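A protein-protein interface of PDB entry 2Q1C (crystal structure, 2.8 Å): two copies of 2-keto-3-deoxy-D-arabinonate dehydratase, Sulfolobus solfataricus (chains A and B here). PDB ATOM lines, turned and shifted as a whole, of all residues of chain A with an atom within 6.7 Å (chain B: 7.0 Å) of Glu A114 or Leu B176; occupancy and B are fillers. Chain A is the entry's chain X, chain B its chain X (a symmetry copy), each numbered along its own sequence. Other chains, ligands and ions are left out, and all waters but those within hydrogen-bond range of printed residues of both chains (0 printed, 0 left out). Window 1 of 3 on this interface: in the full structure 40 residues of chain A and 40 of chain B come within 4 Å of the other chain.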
ATOM      1  N   GLY A  78     -19.806 -33.266   3.134  1.00  0.00           N
ATOM      2  CA  GLY A  78     -20.686 -34.243   3.755  1.00  0.00           C
ATOM      3  C   GLY A  78     -22.123 -33.781   3.846  1.00  0.00           C
ATOM      4  O   GLY A  78     -22.399 -32.582   3.945  1.00  0.00           O
ATOM      5  N   SER A  79     -23.037 -34.745   3.821  1.00  0.00           N
ATOM      6  CA  SER A  79     -24.464 -34.482   3.907  1.00  0.00           C
ATOM      7  C   SER A  79     -25.048 -35.298   5.054  1.00  0.00           C
ATOM      8  O   SER A  79     -24.936 -36.522   5.063  1.00  0.00           O
ATOM      9  CB  SER A  79     -25.138 -34.849   2.586  1.00  0.00           C
ATOM     10  OG  SER A  79     -26.491 -34.440   2.567  1.00  0.00           O
ATOM     11  N   GLY A  80     -25.668 -34.620   6.015  1.00  0.00           N
ATOM     12  CA  GLY A  80     -26.154 -35.271   7.233  1.00  0.00           C
ATOM     13  C   GLY A  80     -27.643 -35.567   7.312  1.00  0.00           C
ATOM     14  O   GLY A  80     -28.461 -34.854   6.728  1.00  0.00           O
ATOM     15  N   ILE A  81     -27.976 -36.627   8.053  1.00  0.00           N
ATOM     16  CA  ILE A  81     -29.360 -37.045   8.351  1.00  0.00           C
ATOM     17  C   ILE A  81     -30.230 -37.171   7.095  1.00  0.00           C
ATOM     18  O   ILE A  81     -31.177 -36.409   6.881  1.00  0.00           O
ATOM     19  CB  ILE A  81     -30.031 -36.141   9.427  1.00  0.00           C
ATOM     20  CG1 ILE A  81     -29.045 -35.835  10.557  1.00  0.00           C
ATOM     21  CG2 ILE A  81     -31.278 -36.812   9.997  1.00  0.00           C
ATOM     22  CD1 ILE A  81     -29.201 -34.455  11.131  1.00  0.00           C
ATOM     23  N   ARG A  89     -30.099 -39.359  16.576  1.00  0.00           N
ATOM     24  CA  ARG A  89     -28.673 -39.110  16.796  1.00  0.00           C
ATOM     25  C   ARG A  89     -28.437 -38.545  18.200  1.00  0.00           C
ATOM     26  O   ARG A  89     -28.584 -37.341  18.432  1.00  0.00           O
ATOM     27  CB  ARG A  89     -28.128 -38.166  15.717  1.00  0.00           C
ATOM     28  CG  ARG A  89     -26.609 -38.128  15.599  1.00  0.00           C
ATOM     29  CD  ARG A  89     -26.185 -37.344  14.369  1.00  0.00           C
ATOM     30  NE  ARG A  89     -24.733 -37.218  14.248  1.00  0.00           N
ATOM     31  CZ  ARG A  89     -23.956 -38.047  13.552  1.00  0.00           C
ATOM     32  NH1 ARG A  89     -24.479 -39.081  12.907  1.00  0.00           N
ATOM     33  NH2 ARG A  89     -22.645 -37.838  13.501  1.00  0.00           N
ATOM     34  N   ILE A 103     -32.596 -30.551  16.994  1.00  0.00           N
ATOM     35  CA  ILE A 103     -32.018 -29.985  15.766  1.00  0.00           C
ATOM     36  C   ILE A 103     -31.866 -31.003  14.635  1.00  0.00           C
ATOM     37  O   ILE A 103     -31.975 -30.654  13.458  1.00  0.00           O
ATOM     38  CB  ILE A 103     -30.657 -29.264  16.016  1.00  0.00           C
ATOM     39  CG1 ILE A 103     -29.629 -30.212  16.647  1.00  0.00           C
ATOM     40  CG2 ILE A 103     -30.858 -28.013  16.869  1.00  0.00           C
ATOM     41  CD1 ILE A 103     -28.184 -29.775  16.467  1.00  0.00           C
ATOM     42  N   TYR A 104     -31.627 -32.259  15.003  1.00  0.00           N
ATOM     43  CA  TYR A 104     -31.430 -33.332  14.034  1.00  0.00           C
ATOM     44  C   TYR A 104     -32.741 -33.762  13.372  1.00  0.00           C
ATOM     45  O   TYR A 104     -32.777 -34.008  12.165  1.00  0.00           O
ATOM     46  CB  TYR A 104     -30.709 -34.524  14.679  1.00  0.00           C
ATOM     47  CG  TYR A 104     -29.337 -34.179  15.222  1.00  0.00           C
ATOM     48  CD1 TYR A 104     -28.225 -34.133  14.384  1.00  0.00           C
ATOM     49  CD2 TYR A 104     -29.153 -33.892  16.573  1.00  0.00           C
ATOM     50  CE1 TYR A 104     -26.966 -33.809  14.871  1.00  0.00           C
ATOM     51  CE2 TYR A 104     -27.894 -33.569  17.074  1.00  0.00           C
ATOM     52  CZ  TYR A 104     -26.808 -33.531  16.216  1.00  0.00           C
ATOM     53  OH  TYR A 104     -25.562 -33.213  16.701  1.00  0.00           O
ATOM     54  N   GLU A 105     -33.814 -33.842  14.156  1.00  0.00           N
ATOM     55  CA  GLU A 105     -35.124 -34.189  13.602  1.00  0.00           C
ATOM     56  C   GLU A 105     -35.797 -32.998  12.911  1.00  0.00           C
ATOM     57  O   GLU A 105     -36.762 -33.170  12.163  1.00  0.00           O
ATOM     58  CB  GLU A 105     -36.035 -34.846  14.653  1.00  0.00           C
ATOM     59  CG  GLU A 105     -36.529 -33.939  15.772  1.00  0.00           C
ATOM     60  CD  GLU A 105     -37.094 -34.713  16.963  1.00  0.00           C
ATOM     61  OE1 GLU A 105     -37.162 -35.964  16.900  1.00  0.00           O
ATOM     62  OE2 GLU A 105     -37.464 -34.068  17.970  1.00  0.00           O
ATOM     63  N   VAL A 107     -33.895 -30.978  10.792  1.00  0.00           N
ATOM     64  CA  VAL A 107     -33.259 -31.063   9.472  1.00  0.00           C
ATOM     65  C   VAL A 107     -33.832 -32.200   8.621  1.00  0.00           C
ATOM     66  O   VAL A 107     -33.956 -32.068   7.401  1.00  0.00           O
ATOM     67  CB  VAL A 107     -31.714 -31.192   9.594  1.00  0.00           C
ATOM     68  CG1 VAL A 107     -31.069 -31.479   8.242  1.00  0.00           C
ATOM     69  CG2 VAL A 107     -31.123 -29.924  10.190  1.00  0.00           C
ATOM     70  N   ARG A 112     -34.459 -27.503   3.490  1.00  0.00           N
ATOM     71  CA  ARG A 112     -33.012 -27.401   3.359  1.00  0.00           C
ATOM     72  C   ARG A 112     -32.331 -28.524   4.144  1.00  0.00           C
ATOM     73  O   ARG A 112     -32.518 -28.627   5.358  1.00  0.00           O
ATOM     74  CB  ARG A 112     -32.546 -26.034   3.866  1.00  0.00           C
ATOM     75  CG  ARG A 112     -31.055 -25.778   3.732  1.00  0.00           C
ATOM     76  CD  ARG A 112     -30.645 -24.473   4.414  1.00  0.00           C
ATOM     77  NE  ARG A 112     -31.253 -23.300   3.789  1.00  0.00           N
ATOM     78  CZ  ARG A 112     -30.798 -22.706   2.688  1.00  0.00           C
ATOM     79  NH1 ARG A 112     -31.430 -21.648   2.204  1.00  0.00           N
ATOM     80  NH2 ARG A 112     -29.720 -23.165   2.065  1.00  0.00           N
ATOM     81  N   PRO A 113     -31.550 -29.376   3.452  1.00  0.00           N
ATOM     82  CA  PRO A 113     -30.815 -30.460   4.106  1.00  0.00           C
ATOM     83  C   PRO A 113     -29.538 -29.965   4.781  1.00  0.00           C
ATOM     84  O   PRO A 113     -29.164 -28.798   4.621  1.00  0.00           O
ATOM     85  CB  PRO A 113     -30.471 -31.393   2.945  1.00  0.00           C
ATOM     86  CG  PRO A 113     -30.343 -30.487   1.774  1.00  0.00           C
ATOM     87  CD  PRO A 113     -31.329 -29.367   1.993  1.00  0.00           C
ATOM     88  N   GLU A 114     -28.883 -30.848   5.533  1.00  0.00           N
ATOM     89  CA  GLU A 114     -27.612 -30.516   6.167  1.00  0.00           C
ATOM     90  C   GLU A 114     -26.442 -30.792   5.223  1.00  0.00           C
ATOM     91  O   GLU A 114     -26.323 -31.886   4.667  1.00  0.00           O
ATOM     92  CB  GLU A 114     -27.428 -31.289   7.473  1.00  0.00           C
ATOM     93  CG  GLU A 114     -26.368 -30.690   8.390  1.00  0.00           C
ATOM     94  CD  GLU A 114     -25.812 -31.682   9.396  1.00  0.00           C
ATOM     95  OE1 GLU A 114     -26.303 -32.831   9.458  1.00  0.00           O
ATOM     96  OE2 GLU A 114     -24.873 -31.304  10.131  1.00  0.00           O
ATOM     97  N   ILE A 115     -25.596 -29.780   5.045  1.00  0.00           N
ATOM     98  CA  ILE A 115     -24.387 -29.885   4.232  1.00  0.00           C
ATOM     99  C   ILE A 115     -23.221 -29.288   5.018  1.00  0.00           C
ATOM    100  O   ILE A 115     -23.308 -28.158   5.514  1.00  0.00           O
ATOM    101  CB  ILE A 115     -24.542 -29.148   2.870  1.00  0.00           C
ATOM    102  CG1 ILE A 115     -25.687 -29.742   2.033  1.00  0.00           C
ATOM    103  CG2 ILE A 115     -23.223 -29.130   2.086  1.00  0.00           C
ATOM    104  CD1 ILE A 115     -25.441 -31.137   1.472  1.00  0.00           C
ATOM    105  N   PHE A 116     -22.140 -30.055   5.140  1.00  0.00           N
ATOM    106  CA  PHE A 116     -20.952 -29.608   5.864  1.00  0.00           C
ATOM    107  C   PHE A 116     -19.666 -29.924   5.108  1.00  0.00           C
ATOM    108  O   PHE A 116     -19.600 -30.901   4.363  1.00  0.00           O
ATOM    109  CB  PHE A 116     -20.914 -30.216   7.276  1.00  0.00           C
ATOM    110  CG  PHE A 116     -20.823 -31.723   7.297  1.00  0.00           C
ATOM    111  CD1 PHE A 116     -19.586 -32.360   7.359  1.00  0.00           C
ATOM    112  CD2 PHE A 116     -21.977 -32.504   7.267  1.00  0.00           C
ATOM    113  CE1 PHE A 116     -19.499 -33.753   7.378  1.00  0.00           C
ATOM    114  CE2 PHE A 116     -21.902 -33.895   7.289  1.00  0.00           C
ATOM    115  CZ  PHE A 116     -20.662 -34.521   7.345  1.00  0.00           C
ATOM    116  N   GLU A 171     -19.430 -33.899  19.469  1.00  0.00           N
ATOM    117  CA  GLU A 171     -20.668 -33.461  18.841  1.00  0.00           C
ATOM    118  C   GLU A 171     -21.803 -33.414  19.868  1.00  0.00           C
ATOM    119  O   GLU A 171     -22.549 -32.435  19.935  1.00  0.00           O
ATOM    120  CB  GLU A 171     -21.018 -34.403  17.683  1.00  0.00           C
ATOM    121  CG  GLU A 171     -22.328 -34.104  16.974  1.00  0.00           C
ATOM    122  CD  GLU A 171     -22.697 -35.159  15.941  1.00  0.00           C
ATOM    123  OE1 GLU A 171     -21.864 -36.050  15.656  1.00  0.00           O
ATOM    124  OE2 GLU A 171     -23.825 -35.097  15.406  1.00  0.00           O
ATOM    125  N   PRO A 175     -23.199 -29.009  19.506  1.00  0.00           N
ATOM    126  CA  PRO A 175     -23.233 -29.083  18.034  1.00  0.00           C
ATOM    127  C   PRO A 175     -22.233 -28.159  17.329  1.00  0.00           C
ATOM    128  O   PRO A 175     -21.872 -28.416  16.182  1.00  0.00           O
ATOM    129  CB  PRO A 175     -24.672 -28.672  17.688  1.00  0.00           C
ATOM    130  CG  PRO A 175     -25.189 -27.978  18.906  1.00  0.00           C
ATOM    131  CD  PRO A 175     -24.516 -28.648  20.060  1.00  0.00           C
ATOM    132  N   LEU A 178     -18.935 -29.608  16.059  1.00  0.00           N
ATOM    133  CA  LEU A 178     -19.024 -30.515  14.914  1.00  0.00           C
ATOM    134  C   LEU A 178     -17.792 -30.453  13.987  1.00  0.00           C
ATOM    135  O   LEU A 178     -17.240 -31.501  13.645  1.00  0.00           O
ATOM    136  CB  LEU A 178     -20.324 -30.281  14.134  1.00  0.00           C
ATOM    137  CG  LEU A 178     -20.778 -31.349  13.135  1.00  0.00           C
ATOM    138  CD1 LEU A 178     -21.627 -32.417  13.807  1.00  0.00           C
ATOM    139  CD2 LEU A 178     -21.550 -30.700  11.992  1.00  0.00           C
ATOM    140  N   ARG A 231     -33.681 -38.508   1.833  1.00  0.00           N
ATOM    141  CA  ARG A 231     -33.158 -37.351   1.115  1.00  0.00           C
ATOM    142  C   ARG A 231     -32.330 -37.816  -0.083  1.00  0.00           C
ATOM    143  O   ARG A 231     -31.260 -38.406   0.081  1.00  0.00           O
ATOM    144  CB  ARG A 231     -32.321 -36.475   2.055  1.00  0.00           C
ATOM    145  CG  ARG A 231     -31.951 -35.107   1.490  1.00  0.00           C
ATOM    146  CD  ARG A 231     -33.054 -34.074   1.691  1.00  0.00           C
ATOM    147  NE  ARG A 231     -33.262 -33.767   3.105  1.00  0.00           N
ATOM    148  CZ  ARG A 231     -33.846 -32.664   3.562  1.00  0.00           C
ATOM    149  NH1 ARG A 231     -33.985 -32.484   4.868  1.00  0.00           N
ATOM    150  NH2 ARG A 231     -34.288 -31.737   2.720  1.00  0.00           N
ATOM    151  N   GLN A 236     -29.163 -33.153  -2.588  1.00  0.00           N
ATOM    152  CA  GLN A 236     -27.972 -32.861  -1.786  1.00  0.00           C
ATOM    153  C   GLN A 236     -26.947 -32.093  -2.617  1.00  0.00           C
ATOM    154  O   GLN A 236     -26.327 -31.146  -2.130  1.00  0.00           O
ATOM    155  CB  GLN A 236     -27.349 -34.151  -1.238  1.00  0.00           C
ATOM    156  CG  GLN A 236     -28.248 -34.965  -0.302  1.00  0.00           C
ATOM    157  CD  GLN A 236     -27.630 -36.299   0.123  1.00  0.00           C
ATOM    158  OE1 GLN A 236     -26.420 -36.504   0.026  1.00  0.00           O
ATOM    159  NE2 GLN A 236     -28.470 -37.207   0.601  1.00  0.00           N
ATOM    160  N   LEU B 170     -29.952 -18.051   8.130  1.00  0.00           N
ATOM    161  CA  LEU B 170     -29.836 -19.502   7.979  1.00  0.00           C
ATOM    162  C   LEU B 170     -29.304 -20.162   9.251  1.00  0.00           C
ATOM    163  O   LEU B 170     -29.700 -21.279   9.596  1.00  0.00           O
ATOM    164  CB  LEU B 170     -28.932 -19.850   6.795  1.00  0.00           C
ATOM    165  CG  LEU B 170     -29.300 -19.318   5.408  1.00  0.00           C
ATOM    166  CD1 LEU B 170     -28.253 -19.757   4.397  1.00  0.00           C
ATOM    167  CD2 LEU B 170     -30.691 -19.775   4.976  1.00  0.00           C
ATOM    168  N   GLU B 171     -28.400 -19.460   9.930  1.00  0.00           N
ATOM    169  CA  GLU B 171     -27.845 -19.896  11.204  1.00  0.00           C
ATOM    170  C   GLU B 171     -28.937 -19.939  12.277  1.00  0.00           C
ATOM    171  O   GLU B 171     -29.050 -20.916  13.020  1.00  0.00           O
ATOM    172  CB  GLU B 171     -26.709 -18.957  11.618  1.00  0.00           C
ATOM    173  CG  GLU B 171     -26.078 -19.254  12.968  1.00  0.00           C
ATOM    174  CD  GLU B 171     -25.065 -18.200  13.395  1.00  0.00           C
ATOM    175  OE1 GLU B 171     -24.731 -17.311  12.578  1.00  0.00           O
ATOM    176  OE2 GLU B 171     -24.598 -18.261  14.553  1.00  0.00           O
ATOM    177  N   GLU B 173     -32.068 -20.228  11.807  1.00  0.00           N
ATOM    178  CA  GLU B 173     -33.022 -21.248  11.395  1.00  0.00           C
ATOM    179  C   GLU B 173     -32.666 -22.612  11.994  1.00  0.00           C
ATOM    180  O   GLU B 173     -33.544 -23.340  12.461  1.00  0.00           O
ATOM    181  CB  GLU B 173     -33.023 -21.325   9.872  1.00  0.00           C
ATOM    182  CG  GLU B 173     -34.340 -21.695   9.235  1.00  0.00           C
ATOM    183  CD  GLU B 173     -34.360 -21.341   7.758  1.00  0.00           C
ATOM    184  OE1 GLU B 173     -34.281 -20.133   7.433  1.00  0.00           O
ATOM    185  OE2 GLU B 173     -34.444 -22.267   6.920  1.00  0.00           O
ATOM    186  N   ASN B 174     -31.373 -22.941  11.971  1.00  0.00           N
ATOM    187  CA  ASN B 174     -30.828 -24.185  12.524  1.00  0.00           C
ATOM    188  C   ASN B 174     -29.301 -24.094  12.534  1.00  0.00           C
ATOM    189  O   ASN B 174     -28.699 -23.796  11.499  1.00  0.00           O
ATOM    190  CB  ASN B 174     -31.282 -25.398  11.699  1.00  0.00           C
ATOM    191  CG  ASN B 174     -31.047 -26.729  12.410  1.00  0.00           C
ATOM    192  OD1 ASN B 174     -29.934 -27.034  12.846  1.00  0.00           O
ATOM    193  ND2 ASN B 174     -32.098 -27.538  12.505  1.00  0.00           N
ATOM    194  N   PRO B 175     -28.666 -24.342  13.700  1.00  0.00           N
ATOM    195  CA  PRO B 175     -27.199 -24.271  13.820  1.00  0.00           C
ATOM    196  C   PRO B 175     -26.439 -25.198  12.865  1.00  0.00           C
ATOM    197  O   PRO B 175     -25.272 -24.945  12.571  1.00  0.00           O
ATOM    198  CB  PRO B 175     -26.937 -24.679  15.277  1.00  0.00           C
ATOM    199  CG  PRO B 175     -28.186 -25.370  15.725  1.00  0.00           C
ATOM    200  CD  PRO B 175     -29.297 -24.699  14.984  1.00  0.00           C
ATOM    201  N   LEU B 176     -27.097 -26.253  12.387  1.00  0.00           N
ATOM    202  CA  LEU B 176     -26.488 -27.198  11.451  1.00  0.00           C
ATOM    203  C   LEU B 176     -26.369 -26.625  10.038  1.00  0.00           C
ATOM    204  O   LEU B 176     -25.712 -27.213   9.177  1.00  0.00           O
ATOM    205  CB  LEU B 176     -27.263 -28.523  11.430  1.00  0.00           C
ATOM    206  CG  LEU B 176     -27.335 -29.352  12.721  1.00  0.00           C
ATOM    207  CD1 LEU B 176     -28.370 -30.462  12.602  1.00  0.00           C
ATOM    208  CD2 LEU B 176     -25.970 -29.929  13.102  1.00  0.00           C
ATOM    209  N   TYR B 177     -27.010 -25.480   9.808  1.00  0.00           N
ATOM    210  CA  TYR B 177     -26.895 -24.764   8.537  1.00  0.00           C
ATOM    211  C   TYR B 177     -25.731 -23.776   8.547  1.00  0.00           C
ATOM    212  O   TYR B 177     -25.522 -23.046   7.577  1.00  0.00           O
ATOM    213  CB  TYR B 177     -28.193 -24.021   8.202  1.00  0.00           C
ATOM    214  CG  TYR B 177     -29.408 -24.893   7.947  1.00  0.00           C
ATOM    215  CD1 TYR B 177     -29.285 -26.162   7.378  1.00  0.00           C
ATOM    216  CD2 TYR B 177     -30.689 -24.426   8.244  1.00  0.00           C
ATOM    217  CE1 TYR B 177     -30.403 -26.950   7.137  1.00  0.00           C
ATOM    218  CE2 TYR B 177     -31.814 -25.204   8.005  1.00  0.00           C
ATOM    219  CZ  TYR B 177     -31.666 -26.464   7.450  1.00  0.00           C
ATOM    220  OH  TYR B 177     -32.780 -27.236   7.211  1.00  0.00           O
ATOM    221  N   LEU B 178     -24.975 -23.759   9.643  1.00  0.00           N
ATOM    222  CA  LEU B 178     -23.836 -22.854   9.797  1.00  0.00           C
ATOM    223  C   LEU B 178     -22.839 -22.920   8.621  1.00  0.00           C
ATOM    224  O   LEU B 178     -22.463 -21.874   8.088  1.00  0.00           O
ATOM    225  CB  LEU B 178     -23.133 -23.086  11.141  1.00  0.00           C
ATOM    226  CG  LEU B 178     -22.160 -22.019  11.650  1.00  0.00           C
ATOM    227  CD1 LEU B 178     -22.878 -20.948  12.457  1.00  0.00           C
ATOM    228  CD2 LEU B 178     -21.065 -22.669  12.489  1.00  0.00           C
ATOM    229  N   PRO B 179     -22.421 -24.142   8.204  1.00  0.00           N
ATOM    230  CA  PRO B 179     -21.517 -24.252   7.050  1.00  0.00           C
ATOM    231  C   PRO B 179     -22.068 -23.617   5.770  1.00  0.00           C
ATOM    232  O   PRO B 179     -21.308 -23.010   5.016  1.00  0.00           O
ATOM    233  CB  PRO B 179     -21.367 -25.766   6.863  1.00  0.00           C
ATOM    234  CG  PRO B 179     -21.659 -26.338   8.186  1.00  0.00           C
ATOM    235  CD  PRO B 179     -22.730 -25.473   8.763  1.00  0.00           C
ATOM    236  N   GLN B 180     -23.371 -23.760   5.534  1.00  0.00           N
ATOM    237  CA  GLN B 180     -24.024 -23.134   4.381  1.00  0.00           C
ATOM    238  C   GLN B 180     -24.058 -21.610   4.522  1.00  0.00           C
ATOM    239  O   GLN B 180     -23.961 -20.886   3.530  1.00  0.00           O
ATOM    240  CB  GLN B 180     -25.442 -23.679   4.186  1.00  0.00           C
ATOM    241  CG  GLN B 180     -25.505 -25.155   3.815  1.00  0.00           C
ATOM    242  CD  GLN B 180     -26.913 -25.619   3.486  1.00  0.00           C
ATOM    243  OE1 GLN B 180     -27.511 -25.184   2.501  1.00  0.00           O
ATOM    244  NE2 GLN B 180     -27.445 -26.519   4.305  1.00  0.00           N
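The backbone carbonyl oxygen of Ile A103 lies within hydrogen-bond range of the side-chain amide nitrogen of Asn B174 (3.3 Å). The guanidinium group of Arg A112 is in hydrogen-bond range of the side-chain amide oxygen of Gln B180. O of Pro A113 sits at hydrogen-bond distance from NE2 of Gln B180, 2.9 Å away. The backbone carbonyl oxygen of Arg A112 lies close to the side-chain hydroxyl of Tyr B177, 2.3 Å away.
3 positions are printed for both chains. Of the 14 pairs that touch across the chains among the printed residues, none has its exchanged pair printed and touching as well.
Leu B176 touches just these residues of chain A: Ile A103 (3.7 Å), Val A107 (3.7 Å) and Glu A114 (3.5 Å). Of the printed residues of chain A, Pro B179 touches Ile A115 (3.4 Å) and Phe A116 (3.99 Å). Of the printed residues of chain A, Pro B175 touches Ile A103 (3.9 Å).
Of the 10 printed residues of chain B, 7 touch a printed residue of chain A. Printed residues of chain B that touch a printed residue of chain A: Leu B170, Asn B174, Pro B175, Leu B176, Tyr B177, Pro B179 and Gln B180. Hydrophobic or aromatic side chains of chain B within 4 Å of the printed part of chain A: Leu B170, Pro B175, Leu B176, Tyr B177 and Pro B179. Of the 19 printed residues of chain A, 7 touch a printed residue of chain B.
Ile A103 touches Pro B175 (CG2 to CG, 3.9 Å). Ile A103 touches Leu B176 (O to CD1, 3.7 Å). Val A107 touches Asn B174. Leu B176 touches Val A107. Leu B170 touches Arg A112 (CD2 to NH1, 3.4 Å). CE1 of Tyr B177 touches O of Pro A113, 3.4 Å away. Leu B176 touches Glu A114 (CD2 to OE2, 3.5 Å). O of Ile A115 touches CB of Pro B179, 3.4 Å away. NE2 of Gln B180 touches N of Ile A115, 3.8 Å away. Pro B179 touches Phe A116 (CB to CA, 3.99 Å).
The backbone carbonyl oxygen (O) of Phe A116 is in hydrogen-bond range of the backbone NH (N) of Gly A78, at 2.7 Å. The backbone carbonyl oxygen (O) of Glu A114 lies close to the side-chain hydroxyl (OG) of Ser A79 (3.3 Å). N of Gly A80 lies within hydrogen-bond range of O of Glu A114, at 3.1 Å. O of Val A107 sits at hydrogen-bond distance from NH1 of Arg A231 (2.6 Å). The backbone NH (N) of Leu B176 sits at hydrogen-bond distance from the side-chain amide oxygen (OD1) of Asn B174, at 3.0 Å.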
